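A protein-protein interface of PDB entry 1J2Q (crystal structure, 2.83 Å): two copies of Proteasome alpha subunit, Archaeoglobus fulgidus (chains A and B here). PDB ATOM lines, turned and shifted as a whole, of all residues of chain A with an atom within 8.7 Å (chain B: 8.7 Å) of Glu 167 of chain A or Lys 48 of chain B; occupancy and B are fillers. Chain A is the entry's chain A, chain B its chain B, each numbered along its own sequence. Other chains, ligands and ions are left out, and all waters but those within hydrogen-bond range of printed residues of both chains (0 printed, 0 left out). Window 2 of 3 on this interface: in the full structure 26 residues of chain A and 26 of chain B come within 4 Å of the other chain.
The backbone NH (N) of Glu 51 of chain B is in hydrogen-bond range of the backbone carbonyl oxygen (O) of Glu 149 of chain A, 2.7 Å away. The side-chain amino group (NZ) of Lys 151 of chain A lies within salt-bridge range of the side-chain carboxylate (OE2) of Glu 51 of chain B. The backbone carbonyl oxygen of Leu 49 of chain B sits at hydrogen-bond distance from the backbone NH of Ala 152 of chain A (3.5 Å). OG of Ser 47 of chain B sits at hydrogen-bond distance from OE1 of Glu 167 of chain A, at 3.2 Å. The backbone NH (N) of Lys 48 of chain B sits close to the side-chain carboxylate (OE2) of Glu 167 of chain A, 3.3 Å away. The backbone NH (N) of Lys 151 of chain A lies close to the backbone carbonyl oxygen (O) of Leu 49 of chain B.
The backbone carbonyl oxygen of Arg 159 of chain A lies within hydrogen-bond range of the side-chain hydroxyl of Thr 163 of chain A (2.8 Å). The side-chain hydroxyl of Ser 47 of chain B sits close to the backbone NH of Leu 49 of chain B (3.1 Å). The side-chain carboxylate (OE1) of Glu 51 of chain B lies close to the side-chain carboxylate (OD2) of Asp 53 of chain B, at 2.5 Å.
Leu 50 of chain B touches Glu 149 of chain A (CA to O, 3.4 Å). Tyr 150 of chain A touches Leu 49 of chain B. CZ of Tyr 150 of chain A touches CD1 of Leu 50 of chain B, at 3.2 Å. Glu 51 of chain B touches Tyr 150 of chain A. Lys 151 of chain A touches Lys 48 of chain B (CD to O, 3.7 Å). Leu 50 of chain B touches Lys 151 of chain A. Thr 163 of chain A touches Leu 49 of chain B. CD2 of Leu 49 of chain B touches CB of Phe 166 of chain A (3.6 Å).
Glu 167 of chain A touches just these residues of chain B: Ser 47 (3.2 Å) and Lys 48 (2.8 Å). Of chain A, only Lys 151 (3.7 Å) and Glu 167 (2.8 Å) come within 4 Å of Lys 48 of chain B. Ser 47 of chain B touches just one residue of chain A: Glu 167 (3.2 Å). Of chain A, only Tyr 150, Lys 151, Ala 152, Thr 163 and Phe 166 come within 4 Å of Leu 49 of chain B. Of the printed residues of chain B, Thr 163 of chain A touches Leu 49. Of the printed residues of chain B, Tyr 150 of chain A touches Leu 49 (3.0 Å), Leu 50 (3.2 Å) and Glu 51 (3.9 Å). Thr 153 of chain A touches none of the printed residues of chain B. The nearest residue of chain B that does not touch Glu 167 of chain A is Leu 49 of chain B (4.1 Å). The nearest printed residue of chain B that does not touch Ala 152 of chain A is Leu 50 of chain B (5.3 Å).
Printed residues of chain B that touch a printed residue of chain A: Ser 47, Lys 48, Leu 49, Leu 50 and Glu 51. Hydrophobic or aromatic side chains of chain B within 4 Å of the printed part of chain A: Leu 49 and Leu 50. Of the 21 printed residues of chain A, 7 touch a printed residue of chain B. Among the printed residues, Asp or Glu carboxylates within 4 Å of a Lys or Arg side-chain nitrogen of the other chain: Lys 151 of chain A with Glu 51 of chain B (3.97 Å).
No position is printed for both chains.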
ATOM      1  N   GLU A 149     -17.280   5.376   3.314  1.00  0.00           N
ATOM      2  CA  GLU A 149     -16.903   5.307   1.907  1.00  0.00           C
ATOM      3  C   GLU A 149     -16.889   3.854   1.451  1.00  0.00           C
ATOM      4  O   GLU A 149     -16.196   3.023   2.022  1.00  0.00           O
ATOM      5  CB  GLU A 149     -15.538   5.919   1.665  1.00  0.00           C
ATOM      6  CG  GLU A 149     -15.216   6.019   0.193  1.00  0.00           C
ATOM      7  CD  GLU A 149     -13.801   6.517  -0.053  1.00  0.00           C
ATOM      8  OE1 GLU A 149     -13.360   6.609  -1.223  1.00  0.00           O
ATOM      9  OE2 GLU A 149     -13.127   6.818   0.940  1.00  0.00           O
ATOM     10  N   TYR A 150     -17.676   3.564   0.425  1.00  0.00           N
ATOM     11  CA  TYR A 150     -17.792   2.222  -0.127  1.00  0.00           C
ATOM     12  C   TYR A 150     -17.225   2.107  -1.547  1.00  0.00           C
ATOM     13  O   TYR A 150     -17.080   3.101  -2.260  1.00  0.00           O
ATOM     14  CB  TYR A 150     -19.270   1.793  -0.180  1.00  0.00           C
ATOM     15  CG  TYR A 150     -19.881   1.413   1.143  1.00  0.00           C
ATOM     16  CD1 TYR A 150     -20.263   2.385   2.061  1.00  0.00           C
ATOM     17  CD2 TYR A 150     -20.105   0.077   1.465  1.00  0.00           C
ATOM     18  CE1 TYR A 150     -20.862   2.036   3.271  1.00  0.00           C
ATOM     19  CE2 TYR A 150     -20.700  -0.286   2.667  1.00  0.00           C
ATOM     20  CZ  TYR A 150     -21.082   0.694   3.567  1.00  0.00           C
ATOM     21  OH  TYR A 150     -21.695   0.328   4.750  1.00  0.00           O
ATOM     22  N   LYS A 151     -16.913   0.875  -1.945  1.00  0.00           N
ATOM     23  CA  LYS A 151     -16.424   0.587  -3.284  1.00  0.00           C
ATOM     24  C   LYS A 151     -17.710   0.305  -4.034  1.00  0.00           C
ATOM     25  O   LYS A 151     -17.866   0.651  -5.210  1.00  0.00           O
ATOM     26  CB  LYS A 151     -15.533  -0.658  -3.300  1.00  0.00           C
ATOM     27  CG  LYS A 151     -14.178  -0.499  -2.620  1.00  0.00           C
ATOM     28  CD  LYS A 151     -13.290  -1.690  -2.959  1.00  0.00           C
ATOM     29  CE  LYS A 151     -11.824  -1.470  -2.587  1.00  0.00           C
ATOM     30  NZ  LYS A 151     -11.603  -1.505  -1.118  1.00  0.00           N
ATOM     31  N   ALA A 152     -18.639  -0.321  -3.320  1.00  0.00           N
ATOM     32  CA  ALA A 152     -19.951  -0.662  -3.863  1.00  0.00           C
ATOM     33  C   ALA A 152     -20.896  -0.942  -2.689  1.00  0.00           C
ATOM     34  O   ALA A 152     -20.468  -1.459  -1.655  1.00  0.00           O
ATOM     35  CB  ALA A 152     -19.845  -1.881  -4.774  1.00  0.00           C
ATOM     36  N   THR A 153     -22.172  -0.585  -2.834  1.00  0.00           N
ATOM     37  CA  THR A 153     -23.117  -0.802  -1.744  1.00  0.00           C
ATOM     38  C   THR A 153     -24.517  -0.407  -2.143  1.00  0.00           C
ATOM     39  O   THR A 153     -24.775  -0.075  -3.305  1.00  0.00           O
ATOM     40  CB  THR A 153     -22.727   0.006  -0.489  1.00  0.00           C
ATOM     41  OG1 THR A 153     -23.653  -0.261   0.564  1.00  0.00           O
ATOM     42  CG2 THR A 153     -22.751   1.489  -0.780  1.00  0.00           C
ATOM     43  N   ARG A 159     -31.374  -3.618   0.335  1.00  0.00           N
ATOM     44  CA  ARG A 159     -29.992  -3.524   0.777  1.00  0.00           C
ATOM     45  C   ARG A 159     -29.247  -4.841   0.844  1.00  0.00           C
ATOM     46  O   ARG A 159     -28.457  -5.152  -0.044  1.00  0.00           O
ATOM     47  CB  ARG A 159     -29.899  -2.837   2.132  1.00  0.00           C
ATOM     48  CG  ARG A 159     -28.469  -2.539   2.522  1.00  0.00           C
ATOM     49  CD  ARG A 159     -28.388  -1.667   3.755  1.00  0.00           C
ATOM     50  NE  ARG A 159     -27.038  -1.142   3.957  1.00  0.00           N
ATOM     51  CZ  ARG A 159     -25.971  -1.888   4.238  1.00  0.00           C
ATOM     52  NH1 ARG A 159     -26.092  -3.211   4.357  1.00  0.00           N
ATOM     53  NH2 ARG A 159     -24.777  -1.318   4.390  1.00  0.00           N
ATOM     54  N   ASN A 160     -29.501  -5.603   1.905  1.00  0.00           N
ATOM     55  CA  ASN A 160     -28.854  -6.904   2.141  1.00  0.00           C
ATOM     56  C   ASN A 160     -28.683  -7.798   0.919  1.00  0.00           C
ATOM     57  O   ASN A 160     -27.621  -8.410   0.737  1.00  0.00           O
ATOM     58  CB  ASN A 160     -29.612  -7.685   3.207  1.00  0.00           C
ATOM     59  CG  ASN A 160     -29.370  -7.148   4.592  1.00  0.00           C
ATOM     60  OD1 ASN A 160     -29.944  -7.639   5.562  1.00  0.00           O
ATOM     61  ND2 ASN A 160     -28.510  -6.132   4.699  1.00  0.00           N
ATOM     62  N   ALA A 161     -29.727  -7.888   0.097  1.00  0.00           N
ATOM     63  CA  ALA A 161     -29.646  -8.710  -1.091  1.00  0.00           C
ATOM     64  C   ALA A 161     -28.426  -8.294  -1.900  1.00  0.00           C
ATOM     65  O   ALA A 161     -27.471  -9.073  -2.050  1.00  0.00           O
ATOM     66  CB  ALA A 161     -30.900  -8.563  -1.918  1.00  0.00           C
ATOM     67  N   VAL A 162     -28.435  -7.052  -2.385  1.00  0.00           N
ATOM     68  CA  VAL A 162     -27.330  -6.570  -3.204  1.00  0.00           C
ATOM     69  C   VAL A 162     -26.013  -6.488  -2.452  1.00  0.00           C
ATOM     70  O   VAL A 162     -24.955  -6.575  -3.056  1.00  0.00           O
ATOM     71  CB  VAL A 162     -27.677  -5.211  -3.890  1.00  0.00           C
ATOM     72  CG1 VAL A 162     -29.114  -4.837  -3.593  1.00  0.00           C
ATOM     73  CG2 VAL A 162     -26.702  -4.133  -3.484  1.00  0.00           C
ATOM     74  N   THR A 163     -26.066  -6.362  -1.137  1.00  0.00           N
ATOM     75  CA  THR A 163     -24.829  -6.293  -0.362  1.00  0.00           C
ATOM     76  C   THR A 163     -24.103  -7.634  -0.406  1.00  0.00           C
ATOM     77  O   THR A 163     -22.885  -7.693  -0.617  1.00  0.00           O
ATOM     78  CB  THR A 163     -25.087  -5.963   1.118  1.00  0.00           C
ATOM     79  OG1 THR A 163     -26.003  -4.865   1.220  1.00  0.00           O
ATOM     80  CG2 THR A 163     -23.789  -5.597   1.802  1.00  0.00           C
ATOM     81  N   GLU A 164     -24.866  -8.708  -0.184  1.00  0.00           N
ATOM     82  CA  GLU A 164     -24.337 -10.082  -0.194  1.00  0.00           C
ATOM     83  C   GLU A 164     -23.835 -10.416  -1.602  1.00  0.00           C
ATOM     84  O   GLU A 164     -22.787 -11.040  -1.770  1.00  0.00           O
ATOM     85  CB  GLU A 164     -25.430 -11.088   0.218  1.00  0.00           C
ATOM     86  N   PHE A 165     -24.588  -9.989  -2.610  1.00  0.00           N
ATOM     87  CA  PHE A 165     -24.206 -10.233  -3.981  1.00  0.00           C
ATOM     88  C   PHE A 165     -22.873  -9.557  -4.289  1.00  0.00           C
ATOM     89  O   PHE A 165     -21.916 -10.228  -4.661  1.00  0.00           O
ATOM     90  CB  PHE A 165     -25.295  -9.725  -4.910  1.00  0.00           C
ATOM     91  CG  PHE A 165     -24.970  -9.875  -6.359  1.00  0.00           C
ATOM     92  CD1 PHE A 165     -24.264  -8.886  -7.031  1.00  0.00           C
ATOM     93  CD2 PHE A 165     -25.392 -10.998  -7.061  1.00  0.00           C
ATOM     94  CE1 PHE A 165     -23.991  -9.009  -8.386  1.00  0.00           C
ATOM     95  CE2 PHE A 165     -25.125 -11.135  -8.421  1.00  0.00           C
ATOM     96  CZ  PHE A 165     -24.423 -10.136  -9.086  1.00  0.00           C
ATOM     97  N   PHE A 166     -22.799  -8.237  -4.127  1.00  0.00           N
ATOM     98  CA  PHE A 166     -21.554  -7.520  -4.392  1.00  0.00           C
ATOM     99  C   PHE A 166     -20.421  -8.122  -3.580  1.00  0.00           C
ATOM    100  O   PHE A 166     -19.270  -8.159  -4.027  1.00  0.00           O
ATOM    101  CB  PHE A 166     -21.659  -6.027  -4.035  1.00  0.00           C
ATOM    102  CG  PHE A 166     -22.445  -5.214  -5.022  1.00  0.00           C
ATOM    103  CD1 PHE A 166     -22.420  -5.517  -6.380  1.00  0.00           C
ATOM    104  CD2 PHE A 166     -23.195  -4.131  -4.595  1.00  0.00           C
ATOM    105  CE1 PHE A 166     -23.134  -4.753  -7.296  1.00  0.00           C
ATOM    106  CE2 PHE A 166     -23.912  -3.358  -5.501  1.00  0.00           C
ATOM    107  CZ  PHE A 166     -23.882  -3.671  -6.856  1.00  0.00           C
ATOM    108  N   GLU A 167     -20.752  -8.581  -2.380  1.00  0.00           N
ATOM    109  CA  GLU A 167     -19.766  -9.171  -1.495  1.00  0.00           C
ATOM    110  C   GLU A 167     -19.013 -10.312  -2.192  1.00  0.00           C
ATOM    111  O   GLU A 167     -17.873 -10.633  -1.838  1.00  0.00           O
ATOM    112  CB  GLU A 167     -20.461  -9.690  -0.240  1.00  0.00           C
ATOM    113  CG  GLU A 167     -19.505 -10.060   0.873  1.00  0.00           C
ATOM    114  CD  GLU A 167     -18.879  -8.844   1.541  1.00  0.00           C
ATOM    115  OE1 GLU A 167     -19.627  -8.100   2.218  1.00  0.00           O
ATOM    116  OE2 GLU A 167     -17.648  -8.636   1.389  1.00  0.00           O
ATOM    117  N   LYS A 168     -19.653 -10.913  -3.191  1.00  0.00           N
ATOM    118  CA  LYS A 168     -19.048 -12.014  -3.925  1.00  0.00           C
ATOM    119  C   LYS A 168     -18.604 -11.634  -5.336  1.00  0.00           C
ATOM    120  O   LYS A 168     -17.479 -11.930  -5.727  1.00  0.00           O
ATOM    121  CB  LYS A 168     -20.026 -13.194  -3.991  1.00  0.00           C
ATOM    122  CG  LYS A 168     -20.190 -13.944  -2.666  1.00  0.00           C
ATOM    123  CD  LYS A 168     -21.299 -15.007  -2.715  1.00  0.00           C
ATOM    124  CE  LYS A 168     -22.694 -14.382  -2.814  1.00  0.00           C
ATOM    125  NZ  LYS A 168     -23.804 -15.356  -2.593  1.00  0.00           N
ATOM    126  N   GLU A 169     -19.478 -10.966  -6.085  1.00  0.00           N
ATOM    127  CA  GLU A 169     -19.189 -10.571  -7.466  1.00  0.00           C
ATOM    128  C   GLU A 169     -18.313  -9.337  -7.714  1.00  0.00           C
ATOM    129  O   GLU A 169     -17.489  -9.325  -8.636  1.00  0.00           O
ATOM    130  CB  GLU A 169     -20.500 -10.392  -8.232  1.00  0.00           C
ATOM    131  CG  GLU A 169     -21.428 -11.586  -8.140  1.00  0.00           C
ATOM    132  CD  GLU A 169     -20.759 -12.892  -8.543  1.00  0.00           C
ATOM    133  OE1 GLU A 169     -21.474 -13.921  -8.609  1.00  0.00           O
ATOM    134  OE2 GLU A 169     -19.528 -12.896  -8.792  1.00  0.00           O
ATOM    135  N   TYR A 170     -18.496  -8.292  -6.915  1.00  0.00           N
ATOM    136  CA  TYR A 170     -17.715  -7.076  -7.102  1.00  0.00           C
ATOM    137  C   TYR A 170     -16.210  -7.322  -7.159  1.00  0.00           C
ATOM    138  O   TYR A 170     -15.674  -8.174  -6.443  1.00  0.00           O
ATOM    139  CB  TYR A 170     -18.003  -6.069  -5.989  1.00  0.00           C
ATOM    140  CG  TYR A 170     -17.228  -4.783  -6.162  1.00  0.00           C
ATOM    141  CD1 TYR A 170     -17.630  -3.825  -7.099  1.00  0.00           C
ATOM    142  CD2 TYR A 170     -16.064  -4.550  -5.430  1.00  0.00           C
ATOM    143  CE1 TYR A 170     -16.886  -2.671  -7.299  1.00  0.00           C
ATOM    144  CE2 TYR A 170     -15.315  -3.404  -5.622  1.00  0.00           C
ATOM    145  CZ  TYR A 170     -15.724  -2.469  -6.556  1.00  0.00           C
ATOM    146  OH  TYR A 170     -14.949  -1.353  -6.758  1.00  0.00           O
ATOM    147  N   ARG A 171     -15.538  -6.547  -8.007  1.00  0.00           N
ATOM    148  CA  ARG A 171     -14.094  -6.648  -8.184  1.00  0.00           C
ATOM    149  C   ARG A 171     -13.502  -5.270  -8.457  1.00  0.00           C
ATOM    150  O   ARG A 171     -14.065  -4.489  -9.232  1.00  0.00           O
ATOM    151  CB  ARG A 171     -13.781  -7.568  -9.357  1.00  0.00           C
ATOM    152  CG  ARG A 171     -14.426  -8.932  -9.264  1.00  0.00           C
ATOM    153  CD  ARG A 171     -14.430  -9.578 -10.629  1.00  0.00           C
ATOM    154  NE  ARG A 171     -13.082  -9.646 -11.183  1.00  0.00           N
ATOM    155  CZ  ARG A 171     -12.792  -9.411 -12.459  1.00  0.00           C
ATOM    156  NH1 ARG A 171     -11.535  -9.497 -12.885  1.00  0.00           N
ATOM    157  NH2 ARG A 171     -13.762  -9.075 -13.306  1.00  0.00           N
ATOM    158  N   ASP A 172     -12.359  -4.990  -7.832  1.00  0.00           N
ATOM    159  CA  ASP A 172     -11.679  -3.703  -7.981  1.00  0.00           C
ATOM    160  C   ASP A 172     -11.346  -3.308  -9.411  1.00  0.00           C
ATOM    161  O   ASP A 172     -11.172  -2.128  -9.701  1.00  0.00           O
ATOM    162  CB  ASP A 172     -10.392  -3.691  -7.157  1.00  0.00           C
ATOM    163  CG  ASP A 172     -10.654  -3.687  -5.663  1.00  0.00           C
ATOM    164  OD1 ASP A 172      -9.689  -3.553  -4.888  1.00  0.00           O
ATOM    165  OD2 ASP A 172     -11.825  -3.817  -5.255  1.00  0.00           O
ATOM    166  N   LEU A 182     -23.246  -5.321 -13.362  1.00  0.00           N
ATOM    167  CA  LEU A 182     -23.205  -5.993 -12.068  1.00  0.00           C
ATOM    168  C   LEU A 182     -24.204  -5.322 -11.133  1.00  0.00           C
ATOM    169  O   LEU A 182     -24.761  -5.957 -10.237  1.00  0.00           O
ATOM    170  CB  LEU A 182     -21.804  -5.902 -11.472  1.00  0.00           C
ATOM    171  CG  LEU A 182     -21.605  -6.697 -10.186  1.00  0.00           C
ATOM    172  CD1 LEU A 182     -21.896  -8.154 -10.460  1.00  0.00           C
ATOM    173  CD2 LEU A 182     -20.176  -6.531  -9.686  1.00  0.00           C
ATOM    174  N   ALA A 186     -27.630  -6.788  -9.373  1.00  0.00           N
ATOM    175  CA  ALA A 186     -27.887  -6.673  -7.938  1.00  0.00           C
ATOM    176  C   ALA A 186     -29.313  -6.176  -7.724  1.00  0.00           C
ATOM    177  O   ALA A 186     -30.018  -6.647  -6.835  1.00  0.00           O
ATOM    178  CB  ALA A 186     -26.890  -5.716  -7.295  1.00  0.00           C
ATOM    179  N   VAL B  45     -12.401  -3.268   8.977  1.00  0.00           N
ATOM    180  CA  VAL B  45     -13.730  -3.110   8.406  1.00  0.00           C
ATOM    181  C   VAL B  45     -14.498  -4.432   8.302  1.00  0.00           C
ATOM    182  O   VAL B  45     -13.898  -5.508   8.301  1.00  0.00           O
ATOM    183  CB  VAL B  45     -13.636  -2.468   6.996  1.00  0.00           C
ATOM    184  CG1 VAL B  45     -12.902  -3.404   6.046  1.00  0.00           C
ATOM    185  CG2 VAL B  45     -15.040  -2.123   6.470  1.00  0.00           C
ATOM    186  N   GLY B  46     -15.824  -4.335   8.191  1.00  0.00           N
ATOM    187  CA  GLY B  46     -16.661  -5.515   8.094  1.00  0.00           C
ATOM    188  C   GLY B  46     -17.212  -5.858   6.720  1.00  0.00           C
ATOM    189  O   GLY B  46     -18.182  -6.618   6.626  1.00  0.00           O
ATOM    190  N   SER B  47     -16.619  -5.310   5.659  1.00  0.00           N
ATOM    191  CA  SER B  47     -17.063  -5.602   4.294  1.00  0.00           C
ATOM    192  C   SER B  47     -16.027  -5.195   3.258  1.00  0.00           C
ATOM    193  O   SER B  47     -15.428  -4.136   3.367  1.00  0.00           O
ATOM    194  CB  SER B  47     -18.375  -4.888   3.997  1.00  0.00           C
ATOM    195  OG  SER B  47     -18.759  -5.083   2.644  1.00  0.00           O
ATOM    196  N   LYS B  48     -15.813  -6.038   2.255  1.00  0.00           N
ATOM    197  CA  LYS B  48     -14.831  -5.728   1.226  1.00  0.00           C
ATOM    198  C   LYS B  48     -15.319  -4.558   0.391  1.00  0.00           C
ATOM    199  O   LYS B  48     -14.571  -4.005  -0.430  1.00  0.00           O
ATOM    200  CB  LYS B  48     -14.565  -6.952   0.330  1.00  0.00           C
ATOM    201  CG  LYS B  48     -15.737  -7.383  -0.562  1.00  0.00           C
ATOM    202  CD  LYS B  48     -15.312  -8.387  -1.662  1.00  0.00           C
ATOM    203  CE  LYS B  48     -15.233  -9.837  -1.159  1.00  0.00           C
ATOM    204  NZ  LYS B  48     -14.185 -10.068  -0.115  1.00  0.00           N
ATOM    205  N   LEU B  49     -16.571  -4.174   0.623  1.00  0.00           N
ATOM    206  CA  LEU B  49     -17.174  -3.081  -0.110  1.00  0.00           C
ATOM    207  C   LEU B  49     -16.802  -1.701   0.420  1.00  0.00           C
ATOM    208  O   LEU B  49     -16.991  -0.714  -0.272  1.00  0.00           O
ATOM    209  CB  LEU B  49     -18.689  -3.266  -0.135  1.00  0.00           C
ATOM    210  CG  LEU B  49     -19.225  -4.194  -1.235  1.00  0.00           C
ATOM    211  CD1 LEU B  49     -18.268  -5.334  -1.492  1.00  0.00           C
ATOM    212  CD2 LEU B  49     -20.597  -4.712  -0.833  1.00  0.00           C
ATOM    213  N   LEU B  50     -16.262  -1.626   1.630  1.00  0.00           N
ATOM    214  CA  LEU B  50     -15.868  -0.337   2.195  1.00  0.00           C
ATOM    215  C   LEU B  50     -14.464   0.043   1.754  1.00  0.00           C
ATOM    216  O   LEU B  50     -13.571  -0.787   1.774  1.00  0.00           O
ATOM    217  CB  LEU B  50     -15.893  -0.375   3.727  1.00  0.00           C
ATOM    218  CG  LEU B  50     -17.205  -0.279   4.519  1.00  0.00           C
ATOM    219  CD1 LEU B  50     -17.951   0.991   4.164  1.00  0.00           C
ATOM    220  CD2 LEU B  50     -18.072  -1.468   4.214  1.00  0.00           C
ATOM    221  N   GLU B  51     -14.268   1.297   1.362  1.00  0.00           N
ATOM    222  CA  GLU B  51     -12.948   1.767   0.953  1.00  0.00           C
ATOM    223  C   GLU B  51     -12.066   1.802   2.182  1.00  0.00           C
ATOM    224  O   GLU B  51     -12.015   2.798   2.890  1.00  0.00           O
ATOM    225  CB  GLU B  51     -13.034   3.177   0.374  1.00  0.00           C
ATOM    226  CG  GLU B  51     -13.374   3.242  -1.104  1.00  0.00           C
ATOM    227  CD  GLU B  51     -12.244   2.724  -1.980  1.00  0.00           C
ATOM    228  OE1 GLU B  51     -11.084   3.127  -1.766  1.00  0.00           O
ATOM    229  OE2 GLU B  51     -12.519   1.922  -2.891  1.00  0.00           O
ATOM    230  N   ALA B  52     -11.366   0.714   2.445  1.00  0.00           N
ATOM    231  CA  ALA B  52     -10.507   0.663   3.616  1.00  0.00           C
ATOM    232  C   ALA B  52      -9.330   1.632   3.528  1.00  0.00           C
ATOM    233  O   ALA B  52      -8.938   2.222   4.532  1.00  0.00           O
ATOM    234  CB  ALA B  52     -10.003  -0.740   3.816  1.00  0.00           C
ATOM    235  N   ASP B  53      -8.763   1.791   2.332  1.00  0.00           N
ATOM    236  CA  ASP B  53      -7.622   2.685   2.142  1.00  0.00           C
ATOM    237  C   ASP B  53      -7.952   4.114   2.561  1.00  0.00           C
ATOM    238  O   ASP B  53      -7.059   4.892   2.893  1.00  0.00           O
ATOM    239  CB  ASP B  53      -7.163   2.662   0.677  1.00  0.00           C
ATOM    240  CG  ASP B  53      -8.316   2.851  -0.305  1.00  0.00           C
ATOM    241  OD1 ASP B  53      -8.043   3.033  -1.515  1.00  0.00           O
ATOM    242  OD2 ASP B  53      -9.492   2.808   0.129  1.00  0.00           O
